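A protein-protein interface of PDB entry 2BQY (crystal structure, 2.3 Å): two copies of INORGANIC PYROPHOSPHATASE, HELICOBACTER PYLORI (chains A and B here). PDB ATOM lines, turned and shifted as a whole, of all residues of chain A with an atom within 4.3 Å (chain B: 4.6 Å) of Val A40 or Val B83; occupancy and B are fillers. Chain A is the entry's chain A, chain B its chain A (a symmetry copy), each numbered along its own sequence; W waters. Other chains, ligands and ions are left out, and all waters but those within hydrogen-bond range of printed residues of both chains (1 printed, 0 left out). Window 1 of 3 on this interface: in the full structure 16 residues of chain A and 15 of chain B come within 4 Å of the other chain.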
ATOM      1  N   LYS A  28       5.161  20.294   8.439  1.00  0.00           N
ATOM      2  CA  LYS A  28       3.952  20.963   8.888  1.00  0.00           C
ATOM      3  C   LYS A  28       2.699  20.493   8.139  1.00  0.00           C
ATOM      4  O   LYS A  28       2.540  20.762   6.941  1.00  0.00           O
ATOM      5  CB  LYS A  28       4.114  22.479   8.727  1.00  0.00           C
ATOM      6  CG  LYS A  28       2.816  23.264   8.837  1.00  0.00           C
ATOM      7  CD  LYS A  28       3.084  24.765   8.904  1.00  0.00           C
ATOM      8  CE  LYS A  28       1.786  25.572   8.817  1.00  0.00           C
ATOM      9  NZ  LYS A  28       0.821  25.221   9.894  1.00  0.00           N
ATOM     10  N   TYR A  29       1.818  19.793   8.857  1.00  0.00           N
ATOM     11  CA  TYR A  29       0.554  19.306   8.297  1.00  0.00           C
ATOM     12  C   TYR A  29      -0.577  20.284   8.638  1.00  0.00           C
ATOM     13  O   TYR A  29      -0.461  21.098   9.565  1.00  0.00           O
ATOM     14  CB  TYR A  29       0.208  17.929   8.870  1.00  0.00           C
ATOM     15  CG  TYR A  29       1.149  16.816   8.439  1.00  0.00           C
ATOM     16  CD1 TYR A  29       0.994  16.197   7.201  1.00  0.00           C
ATOM     17  CD2 TYR A  29       2.192  16.382   9.264  1.00  0.00           C
ATOM     18  CE1 TYR A  29       1.834  15.184   6.795  1.00  0.00           C
ATOM     19  CE2 TYR A  29       3.046  15.371   8.864  1.00  0.00           C
ATOM     20  CZ  TYR A  29       2.865  14.771   7.629  1.00  0.00           C
ATOM     21  OH  TYR A  29       3.718  13.759   7.236  1.00  0.00           O
ATOM     22  N   ALA A  37      -8.921  15.236   5.475  1.00  0.00           N
ATOM     23  CA  ALA A  37      -7.649  14.776   4.928  1.00  0.00           C
ATOM     24  C   ALA A  37      -6.483  15.576   5.499  1.00  0.00           C
ATOM     25  O   ALA A  37      -6.503  16.816   5.500  1.00  0.00           O
ATOM     26  CB  ALA A  37      -7.670  14.893   3.397  1.00  0.00           C
ATOM     27  N   LEU A  38      -5.472  14.854   5.974  1.00  0.00           N
ATOM     28  CA  LEU A  38      -4.295  15.481   6.543  1.00  0.00           C
ATOM     29  C   LEU A  38      -3.477  16.003   5.380  1.00  0.00           C
ATOM     30  O   LEU A  38      -2.926  15.220   4.621  1.00  0.00           O
ATOM     31  CB  LEU A  38      -3.507  14.451   7.350  1.00  0.00           C
ATOM     32  CG  LEU A  38      -2.442  14.974   8.315  1.00  0.00           C
ATOM     33  CD1 LEU A  38      -3.056  16.012   9.255  1.00  0.00           C
ATOM     34  CD2 LEU A  38      -1.853  13.797   9.101  1.00  0.00           C
ATOM     35  N   MET A  39      -3.404  17.322   5.246  1.00  0.00           N
ATOM     36  CA  MET A  39      -2.679  17.967   4.153  1.00  0.00           C
ATOM     37  C   MET A  39      -1.235  18.331   4.502  1.00  0.00           C
ATOM     38  O   MET A  39      -0.952  18.815   5.590  1.00  0.00           O
ATOM     39  CB  MET A  39      -3.421  19.243   3.742  1.00  0.00           C
ATOM     40  CG  MET A  39      -3.855  19.305   2.305  1.00  0.00           C
ATOM     41  SD  MET A  39      -5.017  17.994   1.848  1.00  0.00           S
ATOM     42  CE  MET A  39      -4.636  17.833   0.102  1.00  0.00           C
ATOM     43  N   VAL A  40      -0.332  18.092   3.562  1.00  0.00           N
ATOM     44  CA  VAL A  40       1.065  18.432   3.751  1.00  0.00           C
ATOM     45  C   VAL A  40       1.220  19.891   3.348  1.00  0.00           C
ATOM     46  O   VAL A  40       1.345  20.205   2.190  1.00  0.00           O
ATOM     47  CB  VAL A  40       1.975  17.564   2.865  1.00  0.00           C
ATOM     48  CG1 VAL A  40       3.428  17.970   3.074  1.00  0.00           C
ATOM     49  CG2 VAL A  40       1.775  16.091   3.196  1.00  0.00           C
ATOM     50  N   ASP A  41       1.213  20.785   4.325  1.00  0.00           N
ATOM     51  CA  ASP A  41       1.330  22.219   4.066  1.00  0.00           C
ATOM     52  C   ASP A  41       2.741  22.625   3.664  1.00  0.00           C
ATOM     53  O   ASP A  41       2.905  23.411   2.733  1.00  0.00           O
ATOM     54  CB  ASP A  41       0.875  23.007   5.294  1.00  0.00           C
ATOM     55  CG  ASP A  41       0.429  24.410   4.942  1.00  0.00           C
ATOM     56  OD1 ASP A  41      -0.467  24.557   4.084  1.00  0.00           O
ATOM     57  OD2 ASP A  41       0.978  25.373   5.507  1.00  0.00           O
ATOM     58  N   ARG A  42       3.747  22.112   4.368  1.00  0.00           N
ATOM     59  CA  ARG A  42       5.136  22.416   4.012  1.00  0.00           C
ATOM     60  C   ARG A  42       6.188  21.723   4.850  1.00  0.00           C
ATOM     61  O   ARG A  42       5.888  21.207   5.914  1.00  0.00           O
ATOM     62  CB  ARG A  42       5.397  23.911   4.084  1.00  0.00           C
ATOM     63  CG  ARG A  42       5.655  24.413   5.475  1.00  0.00           C
ATOM     64  CD  ARG A  42       5.971  25.907   5.481  1.00  0.00           C
ATOM     65  NE  ARG A  42       5.054  26.668   4.628  1.00  0.00           N
ATOM     66  CZ  ARG A  42       5.241  26.847   3.321  1.00  0.00           C
ATOM     67  NH1 ARG A  42       4.364  27.538   2.583  1.00  0.00           N
ATOM     68  NH2 ARG A  42       6.344  26.357   2.757  1.00  0.00           N
ATOM     69  N   CYS B  16      -2.417  16.280  -6.718  1.00  0.00           N
ATOM     70  CA  CYS B  16      -2.247  15.779  -5.357  1.00  0.00           C
ATOM     71  C   CYS B  16      -2.056  14.262  -5.317  1.00  0.00           C
ATOM     72  O   CYS B  16      -2.687  13.519  -6.086  1.00  0.00           O
ATOM     73  CB  CYS B  16      -3.439  16.177  -4.474  1.00  0.00           C
ATOM     74  SG  CYS B  16      -4.871  15.196  -4.729  1.00  0.00           S
ATOM     75  N   VAL B  17      -1.181  13.815  -4.419  1.00  0.00           N
ATOM     76  CA  VAL B  17      -0.891  12.396  -4.253  1.00  0.00           C
ATOM     77  C   VAL B  17      -1.269  11.974  -2.839  1.00  0.00           C
ATOM     78  O   VAL B  17      -0.965  12.664  -1.869  1.00  0.00           O
ATOM     79  CB  VAL B  17       0.612  12.092  -4.466  1.00  0.00           C
ATOM     80  CG1 VAL B  17       0.854  10.612  -4.396  1.00  0.00           C
ATOM     81  CG2 VAL B  17       1.076  12.652  -5.793  1.00  0.00           C
ATOM     82  N   VAL B  18      -1.953  10.843  -2.732  1.00  0.00           N
ATOM     83  CA  VAL B  18      -2.349  10.327  -1.429  1.00  0.00           C
ATOM     84  C   VAL B  18      -1.291   9.325  -0.971  1.00  0.00           C
ATOM     85  O   VAL B  18      -1.202   8.225  -1.495  1.00  0.00           O
ATOM     86  CB  VAL B  18      -3.738   9.630  -1.494  1.00  0.00           C
ATOM     87  CG1 VAL B  18      -4.131   9.106  -0.127  1.00  0.00           C
ATOM     88  CG2 VAL B  18      -4.782  10.600  -2.006  1.00  0.00           C
ATOM     89  N   PHE B  78       6.786  11.406   4.345  1.00  0.00           N
ATOM     90  CA  PHE B  78       5.455  11.884   4.663  1.00  0.00           C
ATOM     91  C   PHE B  78       4.651  10.774   5.315  1.00  0.00           C
ATOM     92  O   PHE B  78       4.795   9.603   4.962  1.00  0.00           O
ATOM     93  CB  PHE B  78       4.750  12.375   3.384  1.00  0.00           C
ATOM     94  CG  PHE B  78       5.448  13.524   2.699  1.00  0.00           C
ATOM     95  CD1 PHE B  78       5.686  14.716   3.375  1.00  0.00           C
ATOM     96  CD2 PHE B  78       5.889  13.412   1.386  1.00  0.00           C
ATOM     97  CE1 PHE B  78       6.349  15.759   2.747  1.00  0.00           C
ATOM     98  CE2 PHE B  78       6.552  14.465   0.768  1.00  0.00           C
ATOM     99  CZ  PHE B  78       6.779  15.627   1.455  1.00  0.00           C
ATOM    100  N   GLY B  81      -1.331   8.276   4.744  1.00  0.00           N
ATOM    101  CA  GLY B  81      -2.684   8.761   4.944  1.00  0.00           C
ATOM    102  C   GLY B  81      -2.761  10.248   4.683  1.00  0.00           C
ATOM    103  O   GLY B  81      -3.838  10.811   4.616  1.00  0.00           O
ATOM    104  N   SER B  82      -1.601  10.886   4.565  1.00  0.00           N
ATOM    105  CA  SER B  82      -1.522  12.320   4.308  1.00  0.00           C
ATOM    106  C   SER B  82      -1.567  12.572   2.801  1.00  0.00           C
ATOM    107  O   SER B  82      -1.316  11.678   2.000  1.00  0.00           O
ATOM    108  CB  SER B  82      -0.229  12.903   4.898  1.00  0.00           C
ATOM    109  OG  SER B  82       0.913  12.503   4.173  1.00  0.00           O
ATOM    110  N   VAL B  83      -1.895  13.799   2.422  1.00  0.00           N
ATOM    111  CA  VAL B  83      -1.980  14.159   1.017  1.00  0.00           C
ATOM    112  C   VAL B  83      -0.969  15.238   0.731  1.00  0.00           C
ATOM    113  O   VAL B  83      -0.785  16.139   1.528  1.00  0.00           O
ATOM    114  CB  VAL B  83      -3.399  14.676   0.647  1.00  0.00           C
ATOM    115  CG1 VAL B  83      -3.522  14.815  -0.877  1.00  0.00           C
ATOM    116  CG2 VAL B  83      -4.462  13.721   1.180  1.00  0.00           C
ATOM    117  N   VAL B  84      -0.323  15.158  -0.427  1.00  0.00           N
ATOM    118  CA  VAL B  84       0.685  16.146  -0.797  1.00  0.00           C
ATOM    119  C   VAL B  84       0.552  16.620  -2.241  1.00  0.00           C
ATOM    120  O   VAL B  84       0.471  15.803  -3.163  1.00  0.00           O
ATOM    121  CB  VAL B  84       2.123  15.575  -0.609  1.00  0.00           C
ATOM    122  CG1 VAL B  84       2.299  14.317  -1.455  1.00  0.00           C
ATOM    123  CG2 VAL B  84       3.164  16.620  -0.999  1.00  0.00           C
ATOM    124  N   LYS B  85       0.523  17.939  -2.430  1.00  0.00           N
ATOM    125  CA  LYS B  85       0.440  18.504  -3.768  1.00  0.00           C
ATOM    126  C   LYS B  85       1.826  18.374  -4.386  1.00  0.00           C
ATOM    127  O   LYS B  85       2.814  18.869  -3.827  1.00  0.00           O
ATOM    128  CB  LYS B  85       0.029  19.979  -3.724  1.00  0.00           C
ATOM    129  CG  LYS B  85      -1.422  20.227  -3.323  1.00  0.00           C
ATOM    130  CD  LYS B  85      -1.729  21.724  -3.336  1.00  0.00           C
ATOM    131  CE  LYS B  85      -1.670  22.293  -4.770  1.00  0.00           C
ATOM    132  NZ  LYS B  85      -1.605  23.821  -4.811  1.00  0.00           N
ATOM    133  N   ILE B 112       5.525  23.987  -0.979  1.00  0.00           N
ATOM    134  CA  ILE B 112       5.521  22.986   0.088  1.00  0.00           C
ATOM    135  C   ILE B 112       6.956  22.655   0.508  1.00  0.00           C
ATOM    136  O   ILE B 112       7.320  22.780   1.678  1.00  0.00           O
ATOM    137  CB  ILE B 112       4.820  21.688  -0.365  1.00  0.00           C
ATOM    138  CG1 ILE B 112       3.328  21.948  -0.539  1.00  0.00           C
ATOM    139  CG2 ILE B 112       5.042  20.592   0.652  1.00  0.00           C
ATOM    140  CD1 ILE B 112       2.534  20.720  -0.929  1.00  0.00           C
HETATM  141  O   HOH W   1      -0.600  18.992   0.101  1.00  0.00           O
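Water W1 lies within hydrogen-bond range of N of Lys B85, O of Val A40 and O of Val B83.
Of the 10 printed residues of chain B, 5 touch a printed residue of chain A. Printed residues of chain B that touch a printed residue of chain A: Phe B78, Ser B82, Val B83, Val B84 and Ile B112. Hydrophobic or aromatic side chains of chain B within 4 Å of the printed part of chain A: Phe B78, Val B83, Val B84 and Ile B112. Among the printed residues, 12 pairs touch across the chains.
The backbone NH (N) of Asp A41 is in hydrogen-bond range of the backbone carbonyl oxygen (O) of Lys A28. The backbone NH (N) of Lys A28 is in hydrogen-bond range of the backbone carbonyl oxygen (O) of Arg A42, 2.8 Å away. The backbone NH of Val B17 sits at hydrogen-bond distance from the backbone carbonyl oxygen of Val B84, at 2.9 Å.
The backbone carbonyl oxygen of Leu A38 sits at hydrogen-bond distance from the backbone NH of Val B83, 2.8 Å away. N of Val A40 lies within hydrogen-bond range of O of Val B83, 2.9 Å away.
No position is printed for both chains. Of the 12 pairs that touch across the chains among the printed residues, none has its exchanged pair printed and touching as well.
Among the printed residues, pairs that only touch across the chains: Arg A42 with Ile B112 (3.2 Å), Leu A38 with Ser B82 (3.2 Å), Met A39 with Val B83 (3.4 Å), Val A40 with Ile B112 (3.4 Å), Asp A41 with Ile B112 (3.6 Å), Tyr A29 with Ser B82 (3.6 Å), Tyr A29 with Phe B78 (3.6 Å), Val A40 with Phe B78 (3.7 Å), Val A40 with Ser B82 (3.8 Å) and Val A40 with Val B84 (3.9 Å).
Of the printed residues of chain B, Tyr A29 touches Phe B78 (3.6 Å) and Ser B82 (3.6 Å). Of the printed residues of chain B, Asp A41 touches Ile B112. Val B18 touches none of the printed residues of chain A. Gly B81 touches none of the printed residues of chain A. Val B83 touches just these residues of chain A: Leu A38 (2.8 Å), Met A39 (3.4 Å) and Val A40 (2.9 Å). Of the printed residues of chain A, Val B84 touches Val A40. Of the printed residues of chain A, Ile B112 touches Val A40, Asp A41 and Arg A42. The nearest printed residue of chain B that does not touch Val A40 is Lys B85 (5.2 Å).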
